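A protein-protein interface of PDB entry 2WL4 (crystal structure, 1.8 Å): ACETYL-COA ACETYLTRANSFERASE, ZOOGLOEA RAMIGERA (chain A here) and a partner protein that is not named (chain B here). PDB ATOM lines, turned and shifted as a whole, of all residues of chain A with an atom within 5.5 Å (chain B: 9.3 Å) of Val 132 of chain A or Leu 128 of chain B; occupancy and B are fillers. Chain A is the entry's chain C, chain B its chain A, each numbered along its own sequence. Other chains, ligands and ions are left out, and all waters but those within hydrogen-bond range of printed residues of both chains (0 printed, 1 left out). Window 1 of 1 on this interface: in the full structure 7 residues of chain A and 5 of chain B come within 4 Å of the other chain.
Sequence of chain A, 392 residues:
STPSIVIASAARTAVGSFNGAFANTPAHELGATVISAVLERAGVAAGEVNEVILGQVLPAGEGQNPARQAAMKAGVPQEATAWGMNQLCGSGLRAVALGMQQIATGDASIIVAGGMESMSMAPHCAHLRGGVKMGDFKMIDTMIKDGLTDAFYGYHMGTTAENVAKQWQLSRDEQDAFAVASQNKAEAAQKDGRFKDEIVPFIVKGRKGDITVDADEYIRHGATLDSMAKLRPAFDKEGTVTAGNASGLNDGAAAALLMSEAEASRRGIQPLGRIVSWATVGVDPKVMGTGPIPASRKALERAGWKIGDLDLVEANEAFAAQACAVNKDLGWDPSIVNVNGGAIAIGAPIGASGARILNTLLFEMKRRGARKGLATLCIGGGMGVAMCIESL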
ATOM      1  N   LEU A 128       9.728  22.955  -1.595  1.00  0.00           N
ATOM      2  CA  LEU A 128       8.997  24.190  -1.295  1.00  0.00           C
ATOM      3  C   LEU A 128       9.716  25.470  -1.649  1.00  0.00           C
ATOM      4  O   LEU A 128       9.254  26.561  -1.302  1.00  0.00           O
ATOM      5  CB  LEU A 128       8.657  24.220   0.189  1.00  0.00           C
ATOM      6  CG  LEU A 128       7.711  23.133   0.671  1.00  0.00           C
ATOM      7  CD1 LEU A 128       7.650  23.164   2.187  1.00  0.00           C
ATOM      8  CD2 LEU A 128       6.344  23.367   0.053  1.00  0.00           C
ATOM      9  N   GLY A 130       9.845  26.904  -4.410  1.00  0.00           N
ATOM     10  CA  GLY A 130       9.101  27.699  -5.375  1.00  0.00           C
ATOM     11  C   GLY A 130       8.182  28.719  -4.731  1.00  0.00           C
ATOM     12  O   GLY A 130       8.075  29.854  -5.204  1.00  0.00           O
ATOM     13  N   GLY A 131       7.528  28.322  -3.642  1.00  0.00           N
ATOM     14  CA  GLY A 131       6.576  29.189  -2.972  1.00  0.00           C
ATOM     15  C   GLY A 131       5.214  29.082  -3.628  1.00  0.00           C
ATOM     16  O   GLY A 131       4.812  29.960  -4.388  1.00  0.00           O
ATOM     17  N   VAL A 132       4.508  27.998  -3.328  1.00  0.00           N
ATOM     18  CA  VAL A 132       3.234  27.683  -3.971  1.00  0.00           C
ATOM     19  C   VAL A 132       2.280  28.878  -4.032  1.00  0.00           C
ATOM     20  O   VAL A 132       1.801  29.358  -3.002  1.00  0.00           O
ATOM     21  CB  VAL A 132       2.548  26.496  -3.265  1.00  0.00           C
ATOM     22  CG1 VAL A 132       1.437  25.914  -4.136  1.00  0.00           C
ATOM     23  CG2 VAL A 132       3.576  25.433  -2.931  1.00  0.00           C
ATOM     24  N   LYS A 133       2.002  29.339  -5.249  1.00  0.00           N
ATOM     25  CA  LYS A 133       1.191  30.532  -5.485  1.00  0.00           C
ATOM     26  C   LYS A 133      -0.283  30.340  -5.122  1.00  0.00           C
ATOM     27  O   LYS A 133      -0.919  31.245  -4.573  1.00  0.00           O
ATOM     28  CB  LYS A 133       1.308  30.963  -6.941  1.00  0.00           C
ATOM     29  CG  LYS A 133       0.203  31.889  -7.374  1.00  0.00           C
ATOM     30  CD  LYS A 133      -0.124  31.716  -8.846  1.00  0.00           C
ATOM     31  CE  LYS A 133      -1.549  32.145  -9.114  1.00  0.00           C
ATOM     32  NZ  LYS A 133      -1.676  33.631  -9.122  1.00  0.00           N
ATOM     33  N   MET A 134      -0.829  29.180  -5.475  1.00  0.00           N
ATOM     34  CA  MET A 134      -2.142  28.736  -4.983  1.00  0.00           C
ATOM     35  C   MET A 134      -2.387  27.261  -5.282  1.00  0.00           C
ATOM     36  O   MET A 134      -1.789  26.686  -6.200  1.00  0.00           O
ATOM     37  CB  MET A 134      -3.289  29.578  -5.542  1.00  0.00           C
ATOM     38  CG  MET A 134      -3.714  29.236  -6.965  1.00  0.00           C
ATOM     39  SD  MET A 134      -5.146  30.230  -7.493  1.00  0.00           S
ATOM     40  CE  MET A 134      -5.349  29.648  -9.175  1.00  0.00           C
ATOM     41  N   GLY A 135      -3.277  26.656  -4.503  1.00  0.00           N
ATOM     42  CA  GLY A 135      -3.591  25.244  -4.638  1.00  0.00           C
ATOM     43  C   GLY A 135      -2.849  24.395  -3.619  1.00  0.00           C
ATOM     44  O   GLY A 135      -1.818  24.809  -3.098  1.00  0.00           O
ATOM     45  N   ASP A 136      -3.398  23.226  -3.322  1.00  0.00           N
ATOM     46  CA  ASP A 136      -2.832  22.346  -2.309  1.00  0.00           C
ATOM     47  C   ASP A 136      -1.544  21.785  -2.886  1.00  0.00           C
ATOM     48  O   ASP A 136      -1.370  21.751  -4.101  1.00  0.00           O
ATOM     49  CB  ASP A 136      -3.759  21.181  -1.995  1.00  0.00           C
ATOM     50  CG  ASP A 136      -5.175  21.603  -1.721  1.00  0.00           C
ATOM     51  OD1 ASP A 136      -5.397  22.739  -1.255  1.00  0.00           O
ATOM     52  OD2 ASP A 136      -6.072  20.780  -1.981  1.00  0.00           O
ATOM     53  N   PHE A 137      -0.632  21.375  -2.021  1.00  0.00           N
ATOM     54  CA  PHE A 137       0.517  20.593  -2.467  1.00  0.00           C
ATOM     55  C   PHE A 137       0.699  19.405  -1.535  1.00  0.00           C
ATOM     56  O   PHE A 137       0.271  19.432  -0.381  1.00  0.00           O
ATOM     57  CB  PHE A 137       1.787  21.443  -2.598  1.00  0.00           C
ATOM     58  CG  PHE A 137       2.256  22.058  -1.312  1.00  0.00           C
ATOM     59  CD1 PHE A 137       1.786  23.298  -0.907  1.00  0.00           C
ATOM     60  CD2 PHE A 137       3.183  21.402  -0.512  1.00  0.00           C
ATOM     61  CE1 PHE A 137       2.222  23.869   0.283  1.00  0.00           C
ATOM     62  CE2 PHE A 137       3.623  21.964   0.672  1.00  0.00           C
ATOM     63  CZ  PHE A 137       3.146  23.197   1.070  1.00  0.00           C
ATOM     64  N   HIS B 124      -2.238  23.299  11.697  1.00  0.00           N
ATOM     65  CA  HIS B 124      -1.040  24.115  11.711  1.00  0.00           C
ATOM     66  C   HIS B 124      -0.964  24.767  10.349  1.00  0.00           C
ATOM     67  O   HIS B 124      -1.465  24.215   9.377  1.00  0.00           O
ATOM     68  CB  HIS B 124       0.198  23.244  11.936  1.00  0.00           C
ATOM     69  CG  HIS B 124       0.424  22.876  13.370  1.00  0.00           C
ATOM     70  ND1 HIS B 124      -0.380  21.991  14.041  1.00  0.00           N
ATOM     71  CD2 HIS B 124       1.382  23.270  14.242  1.00  0.00           C
ATOM     72  CE1 HIS B 124       0.069  21.854  15.284  1.00  0.00           C
ATOM     73  NE2 HIS B 124       1.129  22.619  15.428  1.00  0.00           N
ATOM     74  N   CYS B 125      -0.350  25.938  10.261  1.00  0.00           N
ATOM     75  CA  CYS B 125      -0.400  26.662   9.008  1.00  0.00           C
ATOM     76  C   CYS B 125       0.860  27.466   8.723  1.00  0.00           C
ATOM     77  O   CYS B 125       1.721  27.646   9.595  1.00  0.00           O
ATOM     78  CB  CYS B 125      -1.646  27.563   8.955  1.00  0.00           C
ATOM     79  SG  CYS B 125      -1.564  29.072   9.957  1.00  0.00           S
ATOM     80  N   ALA B 126       0.977  27.937   7.489  1.00  0.00           N
ATOM     81  CA  ALA B 126       2.059  28.845   7.141  1.00  0.00           C
ATOM     82  C   ALA B 126       1.745  29.560   5.841  1.00  0.00           C
ATOM     83  O   ALA B 126       1.196  28.966   4.930  1.00  0.00           O
ATOM     84  CB  ALA B 126       3.362  28.086   6.995  1.00  0.00           C
ATOM     85  N   HIS B 127       2.122  30.826   5.754  1.00  0.00           N
ATOM     86  CA  HIS B 127       1.947  31.579   4.508  1.00  0.00           C
ATOM     87  C   HIS B 127       3.102  31.289   3.572  1.00  0.00           C
ATOM     88  O   HIS B 127       4.206  31.777   3.807  1.00  0.00           O
ATOM     89  CB  HIS B 127       1.956  33.068   4.773  1.00  0.00           C
ATOM     90  CG  HIS B 127       1.914  33.895   3.526  1.00  0.00           C
ATOM     91  ND1 HIS B 127       2.869  34.845   3.225  1.00  0.00           N
ATOM     92  CD2 HIS B 127       1.039  33.906   2.491  1.00  0.00           C
ATOM     93  CE1 HIS B 127       2.574  35.416   2.071  1.00  0.00           C
ATOM     94  NE2 HIS B 127       1.468  34.864   1.603  1.00  0.00           N
ATOM     95  N   LEU B 128       2.825  30.550   2.501  1.00  0.00           N
ATOM     96  CA  LEU B 128       3.865  30.012   1.618  1.00  0.00           C
ATOM     97  C   LEU B 128       3.797  30.527   0.175  1.00  0.00           C
ATOM     98  O   LEU B 128       4.480  29.987  -0.705  1.00  0.00           O
ATOM     99  CB  LEU B 128       3.794  28.487   1.620  1.00  0.00           C
ATOM    100  CG  LEU B 128       4.132  27.801   2.956  1.00  0.00           C
ATOM    101  CD1 LEU B 128       3.793  26.328   2.927  1.00  0.00           C
ATOM    102  CD2 LEU B 128       5.603  27.999   3.280  1.00  0.00           C
ATOM    103  N   ARG B 129       2.985  31.558  -0.071  1.00  0.00           N
ATOM    104  CA  ARG B 129       2.862  32.128  -1.417  1.00  0.00           C
ATOM    105  C   ARG B 129       4.046  32.998  -1.794  1.00  0.00           C
ATOM    106  O   ARG B 129       4.453  33.031  -2.954  1.00  0.00           O
ATOM    107  CB  ARG B 129       1.582  32.956  -1.550  1.00  0.00           C
ATOM    108  CG  ARG B 129       0.341  32.133  -1.500  1.00  0.00           C
ATOM    109  CD  ARG B 129      -0.898  32.999  -1.752  1.00  0.00           C
ATOM    110  NE  ARG B 129      -1.947  32.545  -0.867  1.00  0.00           N
ATOM    111  CZ  ARG B 129      -2.693  31.470  -1.084  1.00  0.00           C
ATOM    112  NH1 ARG B 129      -2.527  30.747  -2.186  1.00  0.00           N
ATOM    113  NH2 ARG B 129      -3.615  31.126  -0.202  1.00  0.00           N
ATOM    114  N   GLY B 130       4.574  33.728  -0.819  1.00  0.00           N
ATOM    115  CA  GLY B 130       5.774  34.511  -1.037  1.00  0.00           C
ATOM    116  C   GLY B 130       6.906  33.574  -1.392  1.00  0.00           C
ATOM    117  O   GLY B 130       7.318  33.495  -2.548  1.00  0.00           O
ATOM    118  N   GLY B 131       7.397  32.847  -0.395  1.00  0.00           N
ATOM    119  CA  GLY B 131       8.439  31.863  -0.615  1.00  0.00           C
ATOM    120  C   GLY B 131       9.557  31.918   0.408  1.00  0.00           C
ATOM    121  O   GLY B 131       9.804  32.951   1.027  1.00  0.00           O
ATOM    122  N   VAL B 132      10.227  30.784   0.593  1.00  0.00           N
ATOM    123  CA  VAL B 132      11.386  30.695   1.473  1.00  0.00           C
ATOM    124  C   VAL B 132      12.360  29.695   0.856  1.00  0.00           C
ATOM    125  O   VAL B 132      12.263  28.491   1.090  1.00  0.00           O
ATOM    126  CB  VAL B 132      10.999  30.241   2.898  1.00  0.00           C
ATOM    127  CG1 VAL B 132      12.031  30.719   3.900  1.00  0.00           C
ATOM    128  CG2 VAL B 132       9.618  30.763   3.275  1.00  0.00           C
ATOM    129  N   LYS B 133      13.299  30.203   0.066  1.00  0.00           N
ATOM    130  CA  LYS B 133      14.122  29.356  -0.796  1.00  0.00           C
ATOM    131  C   LYS B 133      15.294  28.642  -0.109  1.00  0.00           C
ATOM    132  O   LYS B 133      16.061  27.937  -0.778  1.00  0.00           O
ATOM    133  CB  LYS B 133      14.613  30.151  -2.015  1.00  0.00           C
ATOM    134  CG  LYS B 133      15.131  31.545  -1.690  1.00  0.00           C
ATOM    135  CD  LYS B 133      13.993  32.560  -1.612  1.00  0.00           C
ATOM    136  CE  LYS B 133      14.296  33.654  -0.604  1.00  0.00           C
ATOM    137  NZ  LYS B 133      13.305  34.768  -0.665  1.00  0.00           N
ATOM    138  N   GLY B 135      16.436  27.223   4.268  1.00  0.00           N
ATOM    139  CA  GLY B 135      16.280  27.248   5.717  1.00  0.00           C
ATOM    140  C   GLY B 135      14.874  26.920   6.241  1.00  0.00           C
ATOM    141  O   GLY B 135      13.889  26.971   5.505  1.00  0.00           O
ATOM    142  N   ASP B 136      14.780  26.577   7.522  1.00  0.00           N
ATOM    143  CA  ASP B 136      13.500  26.187   8.127  1.00  0.00           C
ATOM    144  C   ASP B 136      12.506  27.343   8.165  1.00  0.00           C
ATOM    145  O   ASP B 136      12.896  28.506   8.120  1.00  0.00           O
ATOM    146  CB  ASP B 136      13.695  25.684   9.563  1.00  0.00           C
ATOM    147  CG  ASP B 136      14.935  24.832   9.729  1.00  0.00           C
ATOM    148  OD1 ASP B 136      15.237  24.029   8.826  1.00  0.00           O
ATOM    149  OD2 ASP B 136      15.601  24.953  10.779  1.00  0.00           O
ATOM    150  N   PHE B 137      11.222  27.012   8.269  1.00  0.00           N
ATOM    151  CA  PHE B 137      10.190  28.016   8.535  1.00  0.00           C
ATOM    152  C   PHE B 137       9.232  27.491   9.618  1.00  0.00           C
ATOM    153  O   PHE B 137       9.210  26.294   9.898  1.00  0.00           O
ATOM    154  CB  PHE B 137       9.444  28.429   7.252  1.00  0.00           C
ATOM    155  CG  PHE B 137       8.806  27.282   6.519  1.00  0.00           C
ATOM    156  CD1 PHE B 137       7.517  26.864   6.835  1.00  0.00           C
ATOM    157  CD2 PHE B 137       9.492  26.619   5.515  1.00  0.00           C
ATOM    158  CE1 PHE B 137       6.928  25.807   6.159  1.00  0.00           C
ATOM    159  CE2 PHE B 137       8.914  25.555   4.841  1.00  0.00           C
ATOM    160  CZ  PHE B 137       7.631  25.149   5.159  1.00  0.00           C
ATOM    161  N   LYS B 138       8.469  28.387  10.228  1.00  0.00           N
ATOM    162  CA  LYS B 138       7.523  28.009  11.285  1.00  0.00           C
ATOM    163  C   LYS B 138       6.163  27.551  10.767  1.00  0.00           C
ATOM    164  O   LYS B 138       5.497  28.276  10.024  1.00  0.00           O
ATOM    165  CB  LYS B 138       7.284  29.189  12.227  1.00  0.00           C
ATOM    166  CG  LYS B 138       8.208  29.262  13.418  1.00  0.00           C
ATOM    167  CD  LYS B 138       7.947  30.527  14.226  1.00  0.00           C
ATOM    168  CE  LYS B 138       8.699  30.497  15.548  1.00  0.00           C
ATOM    169  NZ  LYS B 138       8.835  31.851  16.147  1.00  0.00           N
ATOM    170  N   MET B 139       5.749  26.355  11.174  1.00  0.00           N
ATOM    171  CA  MET B 139       4.354  25.965  11.051  1.00  0.00           C
ATOM    172  C   MET B 139       3.653  26.362  12.348  1.00  0.00           C
ATOM    173  O   MET B 139       4.063  25.951  13.440  1.00  0.00           O
ATOM    174  CB  MET B 139       4.214  24.468  10.794  1.00  0.00           C
ATOM    175  CG  MET B 139       4.640  24.044   9.393  1.00  0.00           C
ATOM    176  SD  MET B 139       3.418  24.503   8.140  1.00  0.00           S
ATOM    177  CE  MET B 139       2.258  23.158   8.339  1.00  0.00           C
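The backbone carbonyl oxygen of Leu 128 of chain B sits at hydrogen-bond distance from the backbone NH of Val 132 of chain A (3.3 Å).
The guanidinium group of Arg 129 of chain B is in hydrogen-bond range of the backbone carbonyl oxygen of Lys 133 of chain A, at 2.9 Å.
O of Arg 129 of chain B lies close to O of Gly 131 of chain A (3.4 Å).
CZ of Phe 137 of chain B touches CD1 of Leu 128 of chain A, 3.6 Å away.
Gly 131 of chain A touches Leu 128 of chain B.
O of Val 132 of chain A touches CA of Arg 129 of chain B (3.4 Å).
Arg 129 of chain B touches Met 134 of chain A.
Phe 137 of chain A touches Leu 128 of chain B.
Of the printed residues of chain B, Leu 128 of chain A touches Phe 137 (3.6 Å).
Gly 131 of chain A touches two residues of chain B.
Printed residues of chain B within 4 Å of Lys 133 of chain A: Arg 129.
No residue of chain B comes within 4 Å of Gly 135 of chain A.
Of the printed residues of chain B, Phe 137 of chain A touches Leu 128.
Cys 125 of chain B touches none of the printed residues of chain A.
Of the printed residues of chain A, Arg 129 of chain B touches Gly 131, Val 132, Lys 133 and Met 134.
Lys 133 of chain B touches none of the printed residues of chain A.
Printed residues of chain A within 4 Å of Phe 137 of chain B: Leu 128.
The nearest residue of chain B that does not touch Val 132 of chain A is Gly 130 of chain B (5.6 Å).
The nearest printed residue of chain B that does not touch Met 134 of chain A is Leu 128 of chain B (7.2 Å).
Of the 15 printed residues of chain B, 3 touch a printed residue of chain A.
Hydrophobic or aromatic side chains of chain B that line the printed part of chain A: Leu 128 and Phe 137.
Along chain B the printed residues that touch a printed residue of chain A span positions 128 to 137.
Printed residues of chain A that touch a printed residue of chain B: Leu 128, Gly 131, Val 132, Lys 133, Met 134 and Phe 137.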
